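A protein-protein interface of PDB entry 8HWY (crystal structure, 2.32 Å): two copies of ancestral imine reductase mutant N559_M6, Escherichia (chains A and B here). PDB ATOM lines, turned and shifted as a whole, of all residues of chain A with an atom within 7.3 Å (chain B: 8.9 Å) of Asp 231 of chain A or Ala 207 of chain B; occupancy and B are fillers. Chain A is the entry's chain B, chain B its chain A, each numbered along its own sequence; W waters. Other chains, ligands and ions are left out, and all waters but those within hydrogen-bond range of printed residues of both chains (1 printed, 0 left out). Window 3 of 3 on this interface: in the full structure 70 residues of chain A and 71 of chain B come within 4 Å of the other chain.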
ATOM      1  N   LEU A 223      13.128  10.807  15.003  1.00  0.00           N
ATOM      2  CA  LEU A 223      12.740  12.216  15.057  1.00  0.00           C
ATOM      3  C   LEU A 223      11.281  12.379  15.453  1.00  0.00           C
ATOM      4  O   LEU A 223      10.941  13.200  16.315  1.00  0.00           O
ATOM      5  CB  LEU A 223      12.998  12.890  13.712  1.00  0.00           C
ATOM      6  CG  LEU A 223      14.481  12.931  13.360  1.00  0.00           C
ATOM      7  CD1 LEU A 223      14.817  14.204  12.588  1.00  0.00           C
ATOM      8  CD2 LEU A 223      15.372  12.807  14.603  1.00  0.00           C
ATOM      9  N   GLU A 224      10.395  11.630  14.801  1.00  0.00           N
ATOM     10  CA  GLU A 224       8.990  11.659  15.185  1.00  0.00           C
ATOM     11  C   GLU A 224       8.808  11.189  16.622  1.00  0.00           C
ATOM     12  O   GLU A 224       7.921  11.674  17.335  1.00  0.00           O
ATOM     13  CB  GLU A 224       8.171  10.802  14.216  1.00  0.00           C
ATOM     14  CG  GLU A 224       6.728  11.271  14.025  1.00  0.00           C
ATOM     15  CD  GLU A 224       5.713  10.562  14.968  1.00  0.00           C
ATOM     16  OE1 GLU A 224       6.134   9.725  15.813  1.00  0.00           O
ATOM     17  OE2 GLU A 224       4.488  10.838  14.855  1.00  0.00           O
ATOM     18  N   MET A 226      10.960  11.731  19.102  1.00  0.00           N
ATOM     19  CA  MET A 226      11.309  12.841  19.975  1.00  0.00           C
ATOM     20  C   MET A 226      10.308  13.986  19.898  1.00  0.00           C
ATOM     21  O   MET A 226      10.138  14.711  20.885  1.00  0.00           O
ATOM     22  CB  MET A 226      12.703  13.340  19.635  1.00  0.00           C
ATOM     23  CG  MET A 226      13.743  12.287  19.842  1.00  0.00           C
ATOM     24  SD  MET A 226      15.195  12.686  18.876  1.00  0.00           S
ATOM     25  CE  MET A 226      15.708  14.243  19.580  1.00  0.00           C
ATOM     26  N   ALA A 227       9.659  14.178  18.742  1.00  0.00           N
ATOM     27  CA  ALA A 227       8.631  15.214  18.637  1.00  0.00           C
ATOM     28  C   ALA A 227       7.452  14.900  19.552  1.00  0.00           C
ATOM     29  O   ALA A 227       6.910  15.793  20.216  1.00  0.00           O
ATOM     30  CB  ALA A 227       8.180  15.370  17.179  1.00  0.00           C
ATOM     31  N   GLU A 228       7.066  13.632  19.633  1.00  0.00           N
ATOM     32  CA  GLU A 228       5.985  13.267  20.538  1.00  0.00           C
ATOM     33  C   GLU A 228       6.336  13.658  21.963  1.00  0.00           C
ATOM     34  O   GLU A 228       5.492  14.185  22.705  1.00  0.00           O
ATOM     35  CB  GLU A 228       5.729  11.766  20.439  1.00  0.00           C
ATOM     36  CG  GLU A 228       4.392  11.352  19.871  1.00  0.00           C
ATOM     37  CD  GLU A 228       4.231   9.822  19.854  1.00  0.00           C
ATOM     38  OE1 GLU A 228       5.207   9.113  20.221  1.00  0.00           O
ATOM     39  OE2 GLU A 228       3.129   9.337  19.492  1.00  0.00           O
ATOM     40  N   GLN A 229       7.598  13.433  22.348  1.00  0.00           N
ATOM     41  CA  GLN A 229       8.042  13.736  23.698  1.00  0.00           C
ATOM     42  C   GLN A 229       8.060  15.231  23.918  1.00  0.00           C
ATOM     43  O   GLN A 229       7.555  15.717  24.932  1.00  0.00           O
ATOM     44  CB  GLN A 229       9.424  13.144  23.948  1.00  0.00           C
ATOM     45  CG  GLN A 229       9.390  11.759  24.516  1.00  0.00           C
ATOM     46  CD  GLN A 229      10.766  11.288  24.928  1.00  0.00           C
ATOM     47  OE1 GLN A 229      11.614  12.080  25.343  1.00  0.00           O
ATOM     48  NE2 GLN A 229      10.990   9.990  24.841  1.00  0.00           N
ATOM     49  N   ILE A 230       8.602  15.976  22.942  1.00  0.00           N
ATOM     50  CA  ILE A 230       8.586  17.440  23.002  1.00  0.00           C
ATOM     51  C   ILE A 230       7.161  17.951  23.167  1.00  0.00           C
ATOM     52  O   ILE A 230       6.871  18.768  24.048  1.00  0.00           O
ATOM     53  CB  ILE A 230       9.243  18.049  21.749  1.00  0.00           C
ATOM     54  CG1 ILE A 230      10.761  17.846  21.779  1.00  0.00           C
ATOM     55  CG2 ILE A 230       8.886  19.511  21.673  1.00  0.00           C
ATOM     56  CD1 ILE A 230      11.456  17.951  20.414  1.00  0.00           C
ATOM     57  N   ASP A 231       6.246  17.486  22.317  1.00  0.00           N
ATOM     58  CA  ASP A 231       4.883  17.999  22.392  1.00  0.00           C
ATOM     59  C   ASP A 231       4.205  17.628  23.709  1.00  0.00           C
ATOM     60  O   ASP A 231       3.386  18.405  24.214  1.00  0.00           O
ATOM     61  CB  ASP A 231       4.064  17.496  21.204  1.00  0.00           C
ATOM     62  CG  ASP A 231       4.415  18.219  19.911  1.00  0.00           C
ATOM     63  OD1 ASP A 231       5.132  19.243  20.016  1.00  0.00           O
ATOM     64  OD2 ASP A 231       3.992  17.765  18.809  1.00  0.00           O
ATOM     65  N   ALA A 232       4.517  16.454  24.279  1.00  0.00           N
ATOM     66  CA  ALA A 232       3.981  16.122  25.601  1.00  0.00           C
ATOM     67  C   ALA A 232       4.692  16.853  26.736  1.00  0.00           C
ATOM     68  O   ALA A 232       4.099  17.005  27.807  1.00  0.00           O
ATOM     69  CB  ALA A 232       4.047  14.611  25.877  1.00  0.00           C
ATOM     70  N   GLY A 233       5.934  17.308  26.546  1.00  0.00           N
ATOM     71  CA  GLY A 233       6.708  17.820  27.674  1.00  0.00           C
ATOM     72  C   GLY A 233       7.161  16.756  28.656  1.00  0.00           C
ATOM     73  O   GLY A 233       7.527  17.071  29.798  1.00  0.00           O
ATOM     74  N   GLU A 234       7.145  15.494  28.232  1.00  0.00           N
ATOM     75  CA  GLU A 234       7.479  14.352  29.073  1.00  0.00           C
ATOM     76  C   GLU A 234       8.606  13.585  28.398  1.00  0.00           C
ATOM     77  O   GLU A 234       8.485  13.189  27.236  1.00  0.00           O
ATOM     78  CB  GLU A 234       6.244  13.469  29.290  1.00  0.00           C
ATOM     79  CG  GLU A 234       6.395  12.370  30.330  1.00  0.00           C
ATOM     80  CD  GLU A 234       5.336  11.256  30.172  1.00  0.00           C
ATOM     81  OE1 GLU A 234       4.359  11.251  30.972  1.00  0.00           O
ATOM     82  OE2 GLU A 234       5.488  10.395  29.259  1.00  0.00           O
ATOM     83  N   TYR A 235       9.702  13.376  29.121  1.00  0.00           N
ATOM     84  CA  TYR A 235      10.935  12.873  28.527  1.00  0.00           C
ATOM     85  C   TYR A 235      11.405  11.626  29.258  1.00  0.00           C
ATOM     86  O   TYR A 235      12.391  11.669  30.008  1.00  0.00           O
ATOM     87  CB  TYR A 235      12.002  13.959  28.557  1.00  0.00           C
ATOM     88  CG  TYR A 235      11.503  15.306  28.103  1.00  0.00           C
ATOM     89  CD1 TYR A 235      11.282  15.572  26.756  1.00  0.00           C
ATOM     90  CD2 TYR A 235      11.260  16.314  29.018  1.00  0.00           C
ATOM     91  CE1 TYR A 235      10.854  16.828  26.333  1.00  0.00           C
ATOM     92  CE2 TYR A 235      10.828  17.563  28.610  1.00  0.00           C
ATOM     93  CZ  TYR A 235      10.619  17.815  27.271  1.00  0.00           C
ATOM     94  OH  TYR A 235      10.180  19.060  26.878  1.00  0.00           O
ATOM     95  N   THR A 287      16.023  14.064  24.869  1.00  0.00           N
ATOM     96  CA  THR A 287      15.103  15.037  24.285  1.00  0.00           C
ATOM     97  C   THR A 287      14.819  16.157  25.258  1.00  0.00           C
ATOM     98  O   THR A 287      14.455  17.265  24.843  1.00  0.00           O
ATOM     99  CB  THR A 287      13.786  14.372  23.873  1.00  0.00           C
ATOM    100  OG1 THR A 287      14.051  13.371  22.882  1.00  0.00           O
ATOM    101  CG2 THR A 287      12.758  15.413  23.330  1.00  0.00           C
ATOM    102  N   ARG A 294      14.903  26.422  24.953  1.00  0.00           N
ATOM    103  CA  ARG A 294      13.914  27.489  24.998  1.00  0.00           C
ATOM    104  C   ARG A 294      14.315  28.593  25.950  1.00  0.00           C
ATOM    105  O   ARG A 294      13.694  29.659  25.939  1.00  0.00           O
ATOM    106  CB  ARG A 294      12.563  26.925  25.409  1.00  0.00           C
ATOM    107  CG  ARG A 294      12.150  25.734  24.577  1.00  0.00           C
ATOM    108  CD  ARG A 294      10.771  25.316  24.958  1.00  0.00           C
ATOM    109  NE  ARG A 294      10.264  24.308  24.052  1.00  0.00           N
ATOM    110  CZ  ARG A 294       9.824  23.141  24.474  1.00  0.00           C
ATOM    111  NH1 ARG A 294       9.864  22.822  25.761  1.00  0.00           N
ATOM    112  NH2 ARG A 294       9.293  22.294  23.597  1.00  0.00           N
ATOM    113  N   TYR B 192      18.749  18.962  15.763  1.00  0.00           N
ATOM    114  CA  TYR B 192      17.314  18.771  15.650  1.00  0.00           C
ATOM    115  C   TYR B 192      16.575  19.504  16.756  1.00  0.00           C
ATOM    116  O   TYR B 192      15.600  20.218  16.498  1.00  0.00           O
ATOM    117  CB  TYR B 192      16.985  17.299  15.696  1.00  0.00           C
ATOM    118  CG  TYR B 192      15.514  17.008  15.691  1.00  0.00           C
ATOM    119  CD1 TYR B 192      14.684  17.482  14.663  1.00  0.00           C
ATOM    120  CD2 TYR B 192      14.957  16.209  16.683  1.00  0.00           C
ATOM    121  CE1 TYR B 192      13.338  17.175  14.641  1.00  0.00           C
ATOM    122  CE2 TYR B 192      13.613  15.892  16.674  1.00  0.00           C
ATOM    123  CZ  TYR B 192      12.807  16.371  15.649  1.00  0.00           C
ATOM    124  OH  TYR B 192      11.468  16.048  15.643  1.00  0.00           O
ATOM    125  N   ALA B 196      13.826  22.389  16.633  1.00  0.00           N
ATOM    126  CA  ALA B 196      12.484  22.280  17.186  1.00  0.00           C
ATOM    127  C   ALA B 196      12.208  23.432  18.129  1.00  0.00           C
ATOM    128  O   ALA B 196      11.083  23.933  18.207  1.00  0.00           O
ATOM    129  CB  ALA B 196      12.303  20.949  17.914  1.00  0.00           C
ATOM    130  N   VAL B 199      11.459  26.656  15.876  1.00  0.00           N
ATOM    131  CA  VAL B 199      10.122  26.737  15.325  1.00  0.00           C
ATOM    132  C   VAL B 199       9.087  26.686  16.442  1.00  0.00           C
ATOM    133  O   VAL B 199       8.013  27.296  16.348  1.00  0.00           O
ATOM    134  CB  VAL B 199       9.957  25.617  14.292  1.00  0.00           C
ATOM    135  CG1 VAL B 199       9.446  24.329  14.956  1.00  0.00           C
ATOM    136  CG2 VAL B 199       9.072  26.091  13.189  1.00  0.00           C
ATOM    137  N   GLY B 200       9.409  25.999  17.534  1.00  0.00           N
ATOM    138  CA  GLY B 200       8.493  25.952  18.650  1.00  0.00           C
ATOM    139  C   GLY B 200       8.222  27.316  19.240  1.00  0.00           C
ATOM    140  O   GLY B 200       7.154  27.550  19.801  1.00  0.00           O
ATOM    141  N   GLY B 203       4.907  28.510  18.383  1.00  0.00           N
ATOM    142  CA  GLY B 203       3.756  27.640  18.516  1.00  0.00           C
ATOM    143  C   GLY B 203       3.740  26.453  17.578  1.00  0.00           C
ATOM    144  O   GLY B 203       2.793  25.656  17.620  1.00  0.00           O
ATOM    145  N   VAL B 204       4.770  26.285  16.760  1.00  0.00           N
ATOM    146  CA  VAL B 204       4.804  25.168  15.825  1.00  0.00           C
ATOM    147  C   VAL B 204       5.126  23.915  16.619  1.00  0.00           C
ATOM    148  O   VAL B 204       6.224  23.806  17.187  1.00  0.00           O
ATOM    149  CB  VAL B 204       5.829  25.388  14.706  1.00  0.00           C
ATOM    150  CG1 VAL B 204       5.661  24.314  13.655  1.00  0.00           C
ATOM    151  CG2 VAL B 204       5.680  26.803  14.098  1.00  0.00           C
ATOM    152  N   PRO B 205       4.202  22.964  16.711  1.00  0.00           N
ATOM    153  CA  PRO B 205       4.494  21.741  17.460  1.00  0.00           C
ATOM    154  C   PRO B 205       5.534  20.894  16.747  1.00  0.00           C
ATOM    155  O   PRO B 205       5.539  20.783  15.519  1.00  0.00           O
ATOM    156  CB  PRO B 205       3.139  21.028  17.530  1.00  0.00           C
ATOM    157  CG  PRO B 205       2.361  21.578  16.388  1.00  0.00           C
ATOM    158  CD  PRO B 205       2.803  23.016  16.248  1.00  0.00           C
ATOM    159  N   ALA B 206       6.417  20.283  17.542  1.00  0.00           N
ATOM    160  CA  ALA B 206       7.452  19.418  16.980  1.00  0.00           C
ATOM    161  C   ALA B 206       6.878  18.364  16.031  1.00  0.00           C
ATOM    162  O   ALA B 206       7.516  18.029  15.026  1.00  0.00           O
ATOM    163  CB  ALA B 206       8.248  18.739  18.098  1.00  0.00           C
ATOM    164  N   ALA B 207       5.695  17.808  16.347  1.00  0.00           N
ATOM    165  CA  ALA B 207       5.043  16.850  15.439  1.00  0.00           C
ATOM    166  C   ALA B 207       4.854  17.437  14.037  1.00  0.00           C
ATOM    167  O   ALA B 207       5.111  16.759  13.036  1.00  0.00           O
ATOM    168  CB  ALA B 207       3.696  16.373  16.016  1.00  0.00           C
ATOM    169  N   GLU B 208       4.438  18.707  13.938  1.00  0.00           N
ATOM    170  CA  GLU B 208       4.289  19.326  12.622  1.00  0.00           C
ATOM    171  C   GLU B 208       5.634  19.600  11.956  1.00  0.00           C
ATOM    172  O   GLU B 208       5.723  19.567  10.725  1.00  0.00           O
ATOM    173  CB  GLU B 208       3.486  20.623  12.735  1.00  0.00           C
ATOM    174  CG  GLU B 208       2.112  20.442  13.371  1.00  0.00           C
ATOM    175  CD  GLU B 208       1.121  21.539  12.981  1.00  0.00           C
ATOM    176  OE1 GLU B 208       1.531  22.730  12.893  1.00  0.00           O
ATOM    177  OE2 GLU B 208      -0.070  21.200  12.767  1.00  0.00           O
ATOM    178  N   PHE B 209       6.691  19.855  12.732  1.00  0.00           N
ATOM    179  CA  PHE B 209       7.984  20.178  12.126  1.00  0.00           C
ATOM    180  C   PHE B 209       8.781  18.941  11.733  1.00  0.00           C
ATOM    181  O   PHE B 209       9.507  18.970  10.730  1.00  0.00           O
ATOM    182  CB  PHE B 209       8.813  21.012  13.082  1.00  0.00           C
ATOM    183  CG  PHE B 209      10.186  21.316  12.591  1.00  0.00           C
ATOM    184  CD1 PHE B 209      10.392  22.270  11.614  1.00  0.00           C
ATOM    185  CD2 PHE B 209      11.277  20.676  13.132  1.00  0.00           C
ATOM    186  CE1 PHE B 209      11.693  22.597  11.174  1.00  0.00           C
ATOM    187  CE2 PHE B 209      12.555  20.988  12.716  1.00  0.00           C
ATOM    188  CZ  PHE B 209      12.769  21.953  11.725  1.00  0.00           C
ATOM    189  N   ALA B 210       8.647  17.856  12.496  1.00  0.00           N
ATOM    190  CA  ALA B 210       9.437  16.649  12.255  1.00  0.00           C
ATOM    191  C   ALA B 210       9.446  16.180  10.804  1.00  0.00           C
ATOM    192  O   ALA B 210      10.524  15.784  10.330  1.00  0.00           O
ATOM    193  CB  ALA B 210       8.949  15.515  13.168  1.00  0.00           C
ATOM    194  N   PRO B 211       8.327  16.202  10.049  1.00  0.00           N
ATOM    195  CA  PRO B 211       8.374  15.710   8.651  1.00  0.00           C
ATOM    196  C   PRO B 211       9.272  16.529   7.747  1.00  0.00           C
ATOM    197  O   PRO B 211       9.930  15.960   6.866  1.00  0.00           O
ATOM    198  CB  PRO B 211       6.911  15.776   8.175  1.00  0.00           C
ATOM    199  CG  PRO B 211       6.107  16.370   9.290  1.00  0.00           C
ATOM    200  CD  PRO B 211       6.991  16.686  10.455  1.00  0.00           C
ATOM    201  N   PHE B 212       9.305  17.854   7.915  1.00  0.00           N
ATOM    202  CA  PHE B 212      10.271  18.648   7.166  1.00  0.00           C
ATOM    203  C   PHE B 212      11.689  18.261   7.553  1.00  0.00           C
ATOM    204  O   PHE B 212      12.576  18.190   6.694  1.00  0.00           O
ATOM    205  CB  PHE B 212      10.058  20.153   7.391  1.00  0.00           C
ATOM    206  CG  PHE B 212       8.640  20.624   7.175  1.00  0.00           C
ATOM    207  CD1 PHE B 212       7.609  20.174   7.976  1.00  0.00           C
ATOM    208  CD2 PHE B 212       8.346  21.530   6.182  1.00  0.00           C
ATOM    209  CE1 PHE B 212       6.305  20.595   7.778  1.00  0.00           C
ATOM    210  CE2 PHE B 212       7.042  21.970   5.987  1.00  0.00           C
ATOM    211  CZ  PHE B 212       6.021  21.497   6.791  1.00  0.00           C
ATOM    212  N   ALA B 213      11.922  18.013   8.848  1.00  0.00           N
ATOM    213  CA  ALA B 213      13.268  17.700   9.312  1.00  0.00           C
ATOM    214  C   ALA B 213      13.741  16.395   8.694  1.00  0.00           C
ATOM    215  O   ALA B 213      14.824  16.328   8.098  1.00  0.00           O
ATOM    216  CB  ALA B 213      13.316  17.627  10.845  1.00  0.00           C
ATOM    217  N   THR B 214      12.910  15.357   8.785  1.00  0.00           N
ATOM    218  CA  THR B 214      13.308  14.069   8.242  1.00  0.00           C
ATOM    219  C   THR B 214      13.555  14.185   6.754  1.00  0.00           C
ATOM    220  O   THR B 214      14.490  13.579   6.221  1.00  0.00           O
ATOM    221  CB  THR B 214      12.240  13.020   8.523  1.00  0.00           C
ATOM    222  OG1 THR B 214      11.086  13.335   7.745  1.00  0.00           O
ATOM    223  CG2 THR B 214      11.866  13.011   9.991  1.00  0.00           C
HETATM  224  O   HOH W   1       9.105  23.282  20.917  1.00  0.00           O
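O of Leu 223 of chain A is in hydrogen-bond range of OH of Tyr 192 of chain B, at 3.0 Å. The backbone NH (N) of Ala 206 of chain B lies within hydrogen-bond range of the side-chain carboxylate (OD1) of Asp 231 of chain A (3.0 Å). N of Ala 207 of chain B lies within hydrogen-bond range of OD2 of Asp 231 of chain A (3.0 Å).
O of Pro 211 of chain B is in hydrogen-bond range of OG1 of Thr 214 of chain B, 3.0 Å away.
CG2 of Thr 214 of chain B touches CB of Leu 223 of chain A (3.9 Å). Tyr 192 of chain B touches Met 226 of chain A (CD2 to CE, 3.6 Å). Tyr 192 of chain B touches Ala 227 of chain A. CB of Ala 227 of chain A touches C of Ala 206 of chain B (3.5 Å). Ala 207 of chain B touches Ala 227 of chain A (N to CB, 3.6 Å). Ile 230 of chain A touches Ala 196 of chain B. Ile 230 of chain A touches Ala 206 of chain B. OD2 of Asp 231 of chain A touches CB of Pro 205 of chain B, at 3.6 Å.
Of the printed residues of chain B, Leu 223 of chain A touches Tyr 192 and Thr 214. Of the printed residues of chain B, Ala 227 of chain A touches Tyr 192 (3.7 Å), Ala 206 (3.5 Å) and Ala 207 (3.6 Å). Printed residues of chain B within 4 Å of Ile 230 of chain A: Ala 196 (3.99 Å) and Ala 206 (3.7 Å). Asp 231 of chain A touches three residues of chain B. No residue of chain B comes within 4 Å of Ala 232 of chain A. Printed residues of chain A within 4 Å of Tyr 192 of chain B: Leu 223, Met 226 and Ala 227. Of the printed residues of chain A, Pro 205 of chain B touches Asp 231 (3.6 Å). Phe 212 of chain B touches none of the printed residues of chain A. The nearest printed residue of chain A that does not touch Pro 205 of chain B is Ile 230 of chain A (6.1 Å).
Hydrophobic or aromatic side chains of chain A that line the printed part of chain B: Leu 223, Met 226, Ala 227 and Ile 230. Among the printed residues, no Asp or Glu carboxylate lies within 4 Å of a Lys or Arg side-chain nitrogen of the other chain.
No position is printed for both chains. Of the 11 pairs that touch across the chains among the printed residues, none has its exchanged pair printed and touching as well.
Water W1 bridges the guanidinium group (NH2) of Arg 294 of chain A (2.9 Å) and the backbone carbonyl oxygen (O) of Ala 196 of chain B (3.4 Å).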
